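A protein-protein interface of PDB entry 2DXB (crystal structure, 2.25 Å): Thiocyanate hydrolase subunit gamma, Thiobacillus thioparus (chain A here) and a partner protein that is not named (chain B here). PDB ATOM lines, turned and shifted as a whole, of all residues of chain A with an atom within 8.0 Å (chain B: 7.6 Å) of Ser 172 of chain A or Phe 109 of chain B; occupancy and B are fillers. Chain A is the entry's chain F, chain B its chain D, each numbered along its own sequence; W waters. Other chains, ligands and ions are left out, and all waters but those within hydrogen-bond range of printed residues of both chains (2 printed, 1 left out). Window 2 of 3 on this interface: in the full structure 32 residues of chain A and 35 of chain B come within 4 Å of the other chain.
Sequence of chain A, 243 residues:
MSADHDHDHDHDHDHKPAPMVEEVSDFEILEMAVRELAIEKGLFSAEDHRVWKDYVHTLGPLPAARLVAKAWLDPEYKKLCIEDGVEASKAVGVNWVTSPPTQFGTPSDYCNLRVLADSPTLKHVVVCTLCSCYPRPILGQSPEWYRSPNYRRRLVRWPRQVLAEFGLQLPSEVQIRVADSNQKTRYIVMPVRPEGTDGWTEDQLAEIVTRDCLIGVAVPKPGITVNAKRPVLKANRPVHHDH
ND2 of Asn 111 of chain B sits at hydrogen-bond distance from O of Glu 173 of chain A (3.0 Å).
OD2 of Asp 112 of chain B lies within salt-bridge range of NE of Arg 160 of chain A, at 3.0 Å.
The backbone NH (N) of Ile 176 of chain A lies within hydrogen-bond range of the side-chain carboxylate (OD1) of Asp 112 of chain B, at 3.1 Å.
The side-chain hydroxyl (OG1) of Thr 113 of chain B lies within hydrogen-bond range of the side-chain amide nitrogen (NE2) of Gln 175 of chain A (2.6 Å).
The backbone carbonyl oxygen (O) of Ile 176 of chain A lies within hydrogen-bond range of the backbone NH (N) of Thr 113 of chain B (3.0 Å).
O of Ser 172 of chain A lies close to O of Thr 108 of chain B (3.5 Å).
O of Val 174 of chain A lies close to OD1 of Asp 112 of chain B.
The backbone carbonyl oxygen of Asp 112 of chain B lies within hydrogen-bond range of the backbone NH of Gln 98 of chain B, at 3.0 Å.
The side-chain hydroxyl (OH) of Tyr 105 of chain B is in hydrogen-bond range of the side-chain carboxylate (OD2) of Asp 112 of chain B.
The guanidinium group of Arg 160 of chain A sits at hydrogen-bond distance from the backbone carbonyl oxygen of Leu 170 of chain A, 2.9 Å away.
The backbone carbonyl oxygen (O) of Pro 171 of chain A sits at hydrogen-bond distance from the guanidinium group (NH1) of Arg 160 of chain A (3.2 Å).
NH2 of Arg 160 of chain A lies within hydrogen-bond range of O of Val 174 of chain A (2.8 Å).
The side-chain hydroxyl (OG) of Ser 172 of chain A lies within hydrogen-bond range of the side-chain carboxylate (OE2) of Glu 173 of chain A (2.8 Å).
Of chain B, only Thr 108 (3.5 Å) and Phe 109 (3.7 Å) come within 4 Å of Ser 172 of chain A.
No residue of chain A comes within 4 Å of Ala 110 of chain B.
Of the printed residues of chain B, Pro 159 of chain A touches Gln 98 (3.7 Å) and Tyr 105 (3.6 Å).
Printed residues of chain B within 4 Å of Glu 173 of chain A: Asn 111 (3.0 Å).
Ser 106 of chain B touches none of the printed residues of chain A.
The nearest residue of chain A that does not touch Phe 109 of chain B is Gln 161 of chain A (5.1 Å).
Water W1 lies within hydrogen-bond range of O of Ile 176 of chain A (2.7 Å), O of Thr 113 of chain B (2.9 Å) and NE2 of Gln 98 of chain B (3.1 Å).
Water W2 lies within hydrogen-bond range of N of Arg 160 of chain A (2.8 Å), OH of Tyr 105 of chain B (3.0 Å) and OE1 of Gln 161 of chain A (3.3 Å).
Gln 98 of chain B touches Pro 159 of chain A (NE2 to CG, 3.7 Å).
CG of Pro 159 of chain A touches OH of Tyr 105 of chain B, 3.6 Å away.
Arg 160 of chain A touches Phe 109 of chain B.
Ser 172 of chain A touches Phe 109 of chain B.
CG of Gln 175 of chain A touches O of Asn 111 of chain B, at 3.2 Å.
Printed residues of chain B that touch a printed residue of chain A: Gln 98, Tyr 105, Thr 108, Phe 109, Asn 111, Asp 112 and Thr 113.
Hydrophobic or aromatic side chains of chain B that line the printed part of chain A: Tyr 105 and Phe 109.
Hydrophobic or aromatic side chains of chain A within 4 Å of the printed part of chain B: Pro 159 and Ile 176.
Among the printed residues, Asp or Glu carboxylates within 4 Å of a Lys or Arg side-chain nitrogen of the other chain: Arg 160 of chain A with Asp 112 of chain B.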
ATOM      1  N   PRO A 159     -25.214   9.000 -34.637  1.00  0.00           N
ATOM      2  CA  PRO A 159     -25.603  10.363 -34.256  1.00  0.00           C
ATOM      3  C   PRO A 159     -24.607  11.461 -34.647  1.00  0.00           C
ATOM      4  O   PRO A 159     -25.010  12.536 -35.101  1.00  0.00           O
ATOM      5  CB  PRO A 159     -25.819  10.253 -32.743  1.00  0.00           C
ATOM      6  CG  PRO A 159     -24.869   9.149 -32.342  1.00  0.00           C
ATOM      7  CD  PRO A 159     -25.048   8.140 -33.450  1.00  0.00           C
ATOM      8  N   ARG A 160     -23.316  11.189 -34.484  1.00  0.00           N
ATOM      9  CA  ARG A 160     -22.286  12.168 -34.832  1.00  0.00           C
ATOM     10  C   ARG A 160     -22.377  12.553 -36.306  1.00  0.00           C
ATOM     11  O   ARG A 160     -22.268  13.726 -36.657  1.00  0.00           O
ATOM     12  CB  ARG A 160     -20.894  11.595 -34.541  1.00  0.00           C
ATOM     13  CG  ARG A 160     -20.607  11.347 -33.069  1.00  0.00           C
ATOM     14  CD  ARG A 160     -20.161  12.605 -32.378  1.00  0.00           C
ATOM     15  NE  ARG A 160     -19.900  12.391 -30.957  1.00  0.00           N
ATOM     16  CZ  ARG A 160     -19.388  13.321 -30.159  1.00  0.00           C
ATOM     17  NH1 ARG A 160     -19.080  14.515 -30.654  1.00  0.00           N
ATOM     18  NH2 ARG A 160     -19.203  13.071 -28.867  1.00  0.00           N
ATOM     19  N   GLN A 161     -22.573  11.555 -37.164  1.00  0.00           N
ATOM     20  CA  GLN A 161     -22.678  11.785 -38.600  1.00  0.00           C
ATOM     21  C   GLN A 161     -23.973  12.504 -38.970  1.00  0.00           C
ATOM     22  O   GLN A 161     -23.958  13.464 -39.744  1.00  0.00           O
ATOM     23  CB  GLN A 161     -22.610  10.459 -39.363  1.00  0.00           C
ATOM     24  CG  GLN A 161     -21.237   9.781 -39.389  1.00  0.00           C
ATOM     25  CD  GLN A 161     -20.722   9.379 -38.012  1.00  0.00           C
ATOM     26  OE1 GLN A 161     -21.441   8.782 -37.208  1.00  0.00           O
ATOM     27  NE2 GLN A 161     -19.459   9.692 -37.746  1.00  0.00           N
ATOM     28  N   GLN A 169     -21.765  19.962 -34.646  1.00  0.00           N
ATOM     29  CA  GLN A 169     -20.626  19.147 -34.276  1.00  0.00           C
ATOM     30  C   GLN A 169     -20.253  19.473 -32.835  1.00  0.00           C
ATOM     31  O   GLN A 169     -20.206  20.633 -32.444  1.00  0.00           O
ATOM     32  CB  GLN A 169     -19.465  19.450 -35.225  1.00  0.00           C
ATOM     33  CG  GLN A 169     -18.205  18.652 -34.978  1.00  0.00           C
ATOM     34  CD  GLN A 169     -17.193  18.812 -36.106  1.00  0.00           C
ATOM     35  OE1 GLN A 169     -17.239  18.096 -37.113  1.00  0.00           O
ATOM     36  NE2 GLN A 169     -16.284  19.767 -35.948  1.00  0.00           N
ATOM     37  N   LEU A 170     -20.008  18.440 -32.039  1.00  0.00           N
ATOM     38  CA  LEU A 170     -19.644  18.631 -30.645  1.00  0.00           C
ATOM     39  C   LEU A 170     -18.287  18.010 -30.354  1.00  0.00           C
ATOM     40  O   LEU A 170     -17.839  17.114 -31.072  1.00  0.00           O
ATOM     41  CB  LEU A 170     -20.712  18.014 -29.742  1.00  0.00           C
ATOM     42  CG  LEU A 170     -22.007  18.835 -29.714  1.00  0.00           C
ATOM     43  CD1 LEU A 170     -23.216  17.928 -29.686  1.00  0.00           C
ATOM     44  CD2 LEU A 170     -21.976  19.762 -28.512  1.00  0.00           C
ATOM     45  N   PRO A 171     -17.603  18.497 -29.306  1.00  0.00           N
ATOM     46  CA  PRO A 171     -16.291  17.955 -28.947  1.00  0.00           C
ATOM     47  C   PRO A 171     -16.410  16.448 -28.774  1.00  0.00           C
ATOM     48  O   PRO A 171     -17.440  15.951 -28.311  1.00  0.00           O
ATOM     49  CB  PRO A 171     -15.976  18.660 -27.630  1.00  0.00           C
ATOM     50  CG  PRO A 171     -16.646  19.983 -27.797  1.00  0.00           C
ATOM     51  CD  PRO A 171     -17.980  19.604 -28.409  1.00  0.00           C
ATOM     52  N   SER A 172     -15.364  15.722 -29.146  1.00  0.00           N
ATOM     53  CA  SER A 172     -15.382  14.272 -29.030  1.00  0.00           C
ATOM     54  C   SER A 172     -15.547  13.822 -27.582  1.00  0.00           C
ATOM     55  O   SER A 172     -16.051  12.733 -27.326  1.00  0.00           O
ATOM     56  CB  SER A 172     -14.095  13.679 -29.610  1.00  0.00           C
ATOM     57  OG  SER A 172     -12.960  14.147 -28.903  1.00  0.00           O
ATOM     58  N   GLU A 173     -15.128  14.665 -26.642  1.00  0.00           N
ATOM     59  CA  GLU A 173     -15.229  14.331 -25.227  1.00  0.00           C
ATOM     60  C   GLU A 173     -16.654  14.472 -24.708  1.00  0.00           C
ATOM     61  O   GLU A 173     -17.046  13.772 -23.776  1.00  0.00           O
ATOM     62  CB  GLU A 173     -14.310  15.224 -24.392  1.00  0.00           C
ATOM     63  CG  GLU A 173     -12.974  15.533 -25.047  1.00  0.00           C
ATOM     64  CD  GLU A 173     -13.079  16.661 -26.060  1.00  0.00           C
ATOM     65  OE1 GLU A 173     -13.449  17.784 -25.657  1.00  0.00           O
ATOM     66  OE2 GLU A 173     -12.790  16.427 -27.252  1.00  0.00           O
ATOM     67  N   VAL A 174     -17.421  15.382 -25.300  1.00  0.00           N
ATOM     68  CA  VAL A 174     -18.805  15.592 -24.881  1.00  0.00           C
ATOM     69  C   VAL A 174     -19.628  14.324 -25.095  1.00  0.00           C
ATOM     70  O   VAL A 174     -19.480  13.631 -26.102  1.00  0.00           O
ATOM     71  CB  VAL A 174     -19.456  16.749 -25.670  1.00  0.00           C
ATOM     72  CG1 VAL A 174     -20.962  16.789 -25.420  1.00  0.00           C
ATOM     73  CG2 VAL A 174     -18.827  18.065 -25.258  1.00  0.00           C
ATOM     74  N   GLN A 175     -20.482  14.011 -24.131  1.00  0.00           N
ATOM     75  CA  GLN A 175     -21.330  12.841 -24.256  1.00  0.00           C
ATOM     76  C   GLN A 175     -22.557  13.199 -25.084  1.00  0.00           C
ATOM     77  O   GLN A 175     -23.362  14.036 -24.674  1.00  0.00           O
ATOM     78  CB  GLN A 175     -21.789  12.350 -22.876  1.00  0.00           C
ATOM     79  CG  GLN A 175     -23.010  11.425 -22.923  1.00  0.00           C
ATOM     80  CD  GLN A 175     -23.439  10.931 -21.551  1.00  0.00           C
ATOM     81  OE1 GLN A 175     -23.017  11.463 -20.527  1.00  0.00           O
ATOM     82  NE2 GLN A 175     -24.290   9.917 -21.527  1.00  0.00           N
ATOM     83  N   ILE A 176     -22.683  12.605 -26.265  1.00  0.00           N
ATOM     84  CA  ILE A 176     -23.869  12.843 -27.075  1.00  0.00           C
ATOM     85  C   ILE A 176     -24.796  11.714 -26.642  1.00  0.00           C
ATOM     86  O   ILE A 176     -24.411  10.544 -26.680  1.00  0.00           O
ATOM     87  CB  ILE A 176     -23.599  12.719 -28.603  1.00  0.00           C
ATOM     88  CG1 ILE A 176     -23.074  14.041 -29.173  1.00  0.00           C
ATOM     89  CG2 ILE A 176     -24.894  12.371 -29.330  1.00  0.00           C
ATOM     90  CD1 ILE A 176     -21.832  14.545 -28.505  1.00  0.00           C
ATOM     91  N   GLN B  98     -22.913   3.545 -26.261  1.00  0.00           N
ATOM     92  CA  GLN B  98     -23.028   3.290 -27.696  1.00  0.00           C
ATOM     93  C   GLN B  98     -22.133   2.154 -28.169  1.00  0.00           C
ATOM     94  O   GLN B  98     -22.509   1.392 -29.063  1.00  0.00           O
ATOM     95  CB  GLN B  98     -22.723   4.565 -28.490  1.00  0.00           C
ATOM     96  CG  GLN B  98     -23.849   5.590 -28.454  1.00  0.00           C
ATOM     97  CD  GLN B  98     -24.999   5.234 -29.390  1.00  0.00           C
ATOM     98  OE1 GLN B  98     -25.479   4.098 -29.408  1.00  0.00           O
ATOM     99  NE2 GLN B  98     -25.447   6.211 -30.172  1.00  0.00           N
ATOM    100  N   LYS B  99     -20.959   2.029 -27.558  1.00  0.00           N
ATOM    101  CA  LYS B  99     -20.011   0.986 -27.939  1.00  0.00           C
ATOM    102  C   LYS B  99     -20.539  -0.416 -27.644  1.00  0.00           C
ATOM    103  O   LYS B  99     -20.130  -1.385 -28.284  1.00  0.00           O
ATOM    104  CB  LYS B  99     -18.675   1.193 -27.220  1.00  0.00           C
ATOM    105  CG  LYS B  99     -18.789   1.141 -25.704  1.00  0.00           C
ATOM    106  CD  LYS B  99     -17.432   1.225 -25.031  1.00  0.00           C
ATOM    107  CE  LYS B  99     -17.565   1.061 -23.521  1.00  0.00           C
ATOM    108  NZ  LYS B  99     -18.170  -0.255 -23.142  1.00  0.00           N
ATOM    109  N   TYR B 105     -18.461   1.334 -33.269  1.00  0.00           N
ATOM    110  CA  TYR B 105     -18.392   2.671 -32.678  1.00  0.00           C
ATOM    111  C   TYR B 105     -16.949   3.057 -32.363  1.00  0.00           C
ATOM    112  O   TYR B 105     -16.188   2.266 -31.801  1.00  0.00           O
ATOM    113  CB  TYR B 105     -19.244   2.761 -31.411  1.00  0.00           C
ATOM    114  CG  TYR B 105     -19.928   4.104 -31.272  1.00  0.00           C
ATOM    115  CD1 TYR B 105     -21.056   4.406 -32.031  1.00  0.00           C
ATOM    116  CD2 TYR B 105     -19.411   5.097 -30.433  1.00  0.00           C
ATOM    117  CE1 TYR B 105     -21.655   5.662 -31.970  1.00  0.00           C
ATOM    118  CE2 TYR B 105     -20.004   6.365 -30.365  1.00  0.00           C
ATOM    119  CZ  TYR B 105     -21.126   6.637 -31.138  1.00  0.00           C
ATOM    120  OH  TYR B 105     -21.720   7.882 -31.095  1.00  0.00           O
ATOM    121  N   SER B 106     -16.581   4.280 -32.726  1.00  0.00           N
ATOM    122  CA  SER B 106     -15.226   4.782 -32.525  1.00  0.00           C
ATOM    123  C   SER B 106     -14.847   5.107 -31.077  1.00  0.00           C
ATOM    124  O   SER B 106     -15.613   5.745 -30.350  1.00  0.00           O
ATOM    125  CB  SER B 106     -15.018   6.029 -33.388  1.00  0.00           C
ATOM    126  OG  SER B 106     -13.766   6.630 -33.119  1.00  0.00           O
ATOM    127  N   ASP B 107     -13.649   4.685 -30.672  1.00  0.00           N
ATOM    128  CA  ASP B 107     -13.166   4.962 -29.320  1.00  0.00           C
ATOM    129  C   ASP B 107     -13.055   6.468 -29.091  1.00  0.00           C
ATOM    130  O   ASP B 107     -13.060   6.930 -27.949  1.00  0.00           O
ATOM    131  CB  ASP B 107     -11.789   4.330 -29.080  1.00  0.00           C
ATOM    132  CG  ASP B 107     -11.821   2.820 -29.120  1.00  0.00           C
ATOM    133  OD1 ASP B 107     -12.803   2.224 -28.621  1.00  0.00           O
ATOM    134  OD2 ASP B 107     -10.851   2.229 -29.640  1.00  0.00           O
ATOM    135  N   THR B 108     -12.945   7.227 -30.177  1.00  0.00           N
ATOM    136  CA  THR B 108     -12.844   8.680 -30.082  1.00  0.00           C
ATOM    137  C   THR B 108     -14.073   9.274 -29.396  1.00  0.00           C
ATOM    138  O   THR B 108     -13.982  10.290 -28.712  1.00  0.00           O
ATOM    139  CB  THR B 108     -12.704   9.319 -31.477  1.00  0.00           C
ATOM    140  OG1 THR B 108     -11.496   8.856 -32.089  1.00  0.00           O
ATOM    141  CG2 THR B 108     -12.664  10.839 -31.377  1.00  0.00           C
ATOM    142  N   PHE B 109     -15.222   8.632 -29.582  1.00  0.00           N
ATOM    143  CA  PHE B 109     -16.465   9.107 -28.983  1.00  0.00           C
ATOM    144  C   PHE B 109     -16.932   8.128 -27.910  1.00  0.00           C
ATOM    145  O   PHE B 109     -18.122   7.834 -27.784  1.00  0.00           O
ATOM    146  CB  PHE B 109     -17.523   9.253 -30.074  1.00  0.00           C
ATOM    147  CG  PHE B 109     -17.054  10.058 -31.250  1.00  0.00           C
ATOM    148  CD1 PHE B 109     -16.678  11.392 -31.091  1.00  0.00           C
ATOM    149  CD2 PHE B 109     -16.963   9.481 -32.516  1.00  0.00           C
ATOM    150  CE1 PHE B 109     -16.219  12.139 -32.167  1.00  0.00           C
ATOM    151  CE2 PHE B 109     -16.504  10.222 -33.602  1.00  0.00           C
ATOM    152  CZ  PHE B 109     -16.129  11.555 -33.428  1.00  0.00           C
ATOM    153  N   ALA B 110     -15.973   7.644 -27.130  1.00  0.00           N
ATOM    154  CA  ALA B 110     -16.228   6.674 -26.067  1.00  0.00           C
ATOM    155  C   ALA B 110     -17.271   7.060 -25.021  1.00  0.00           C
ATOM    156  O   ALA B 110     -17.724   6.206 -24.269  1.00  0.00           O
ATOM    157  CB  ALA B 110     -14.917   6.329 -25.372  1.00  0.00           C
ATOM    158  N   ASN B 111     -17.656   8.329 -24.956  1.00  0.00           N
ATOM    159  CA  ASN B 111     -18.644   8.734 -23.960  1.00  0.00           C
ATOM    160  C   ASN B 111     -20.095   8.793 -24.451  1.00  0.00           C
ATOM    161  O   ASN B 111     -21.002   9.060 -23.662  1.00  0.00           O
ATOM    162  CB  ASN B 111     -18.262  10.092 -23.354  1.00  0.00           C
ATOM    163  CG  ASN B 111     -16.922  10.056 -22.627  1.00  0.00           C
ATOM    164  OD1 ASN B 111     -16.631   9.122 -21.876  1.00  0.00           O
ATOM    165  ND2 ASN B 111     -16.108  11.084 -22.835  1.00  0.00           N
ATOM    166  N   ASP B 112     -20.326   8.538 -25.737  1.00  0.00           N
ATOM    167  CA  ASP B 112     -21.685   8.592 -26.273  1.00  0.00           C
ATOM    168  C   ASP B 112     -22.592   7.489 -25.739  1.00  0.00           C
ATOM    169  O   ASP B 112     -22.180   6.336 -25.582  1.00  0.00           O
ATOM    170  CB  ASP B 112     -21.657   8.558 -27.802  1.00  0.00           C
ATOM    171  CG  ASP B 112     -21.007   9.796 -28.399  1.00  0.00           C
ATOM    172  OD1 ASP B 112     -20.683  10.729 -27.631  1.00  0.00           O
ATOM    173  OD2 ASP B 112     -20.824   9.841 -29.635  1.00  0.00           O
ATOM    174  N   THR B 113     -23.840   7.854 -25.469  1.00  0.00           N
ATOM    175  CA  THR B 113     -24.814   6.917 -24.932  1.00  0.00           C
ATOM    176  C   THR B 113     -26.159   6.992 -25.644  1.00  0.00           C
ATOM    177  O   THR B 113     -26.395   7.845 -26.505  1.00  0.00           O
ATOM    178  CB  THR B 113     -25.094   7.198 -23.451  1.00  0.00           C
ATOM    179  OG1 THR B 113     -25.558   8.544 -23.319  1.00  0.00           O
ATOM    180  CG2 THR B 113     -23.834   7.014 -22.609  1.00  0.00           C
HETATM  181  O   HOH W   1     -24.941   8.874 -28.730  1.00  0.00           O
HETATM  182  O   HOH W   2     -21.773   8.887 -33.893  1.00  0.00           O
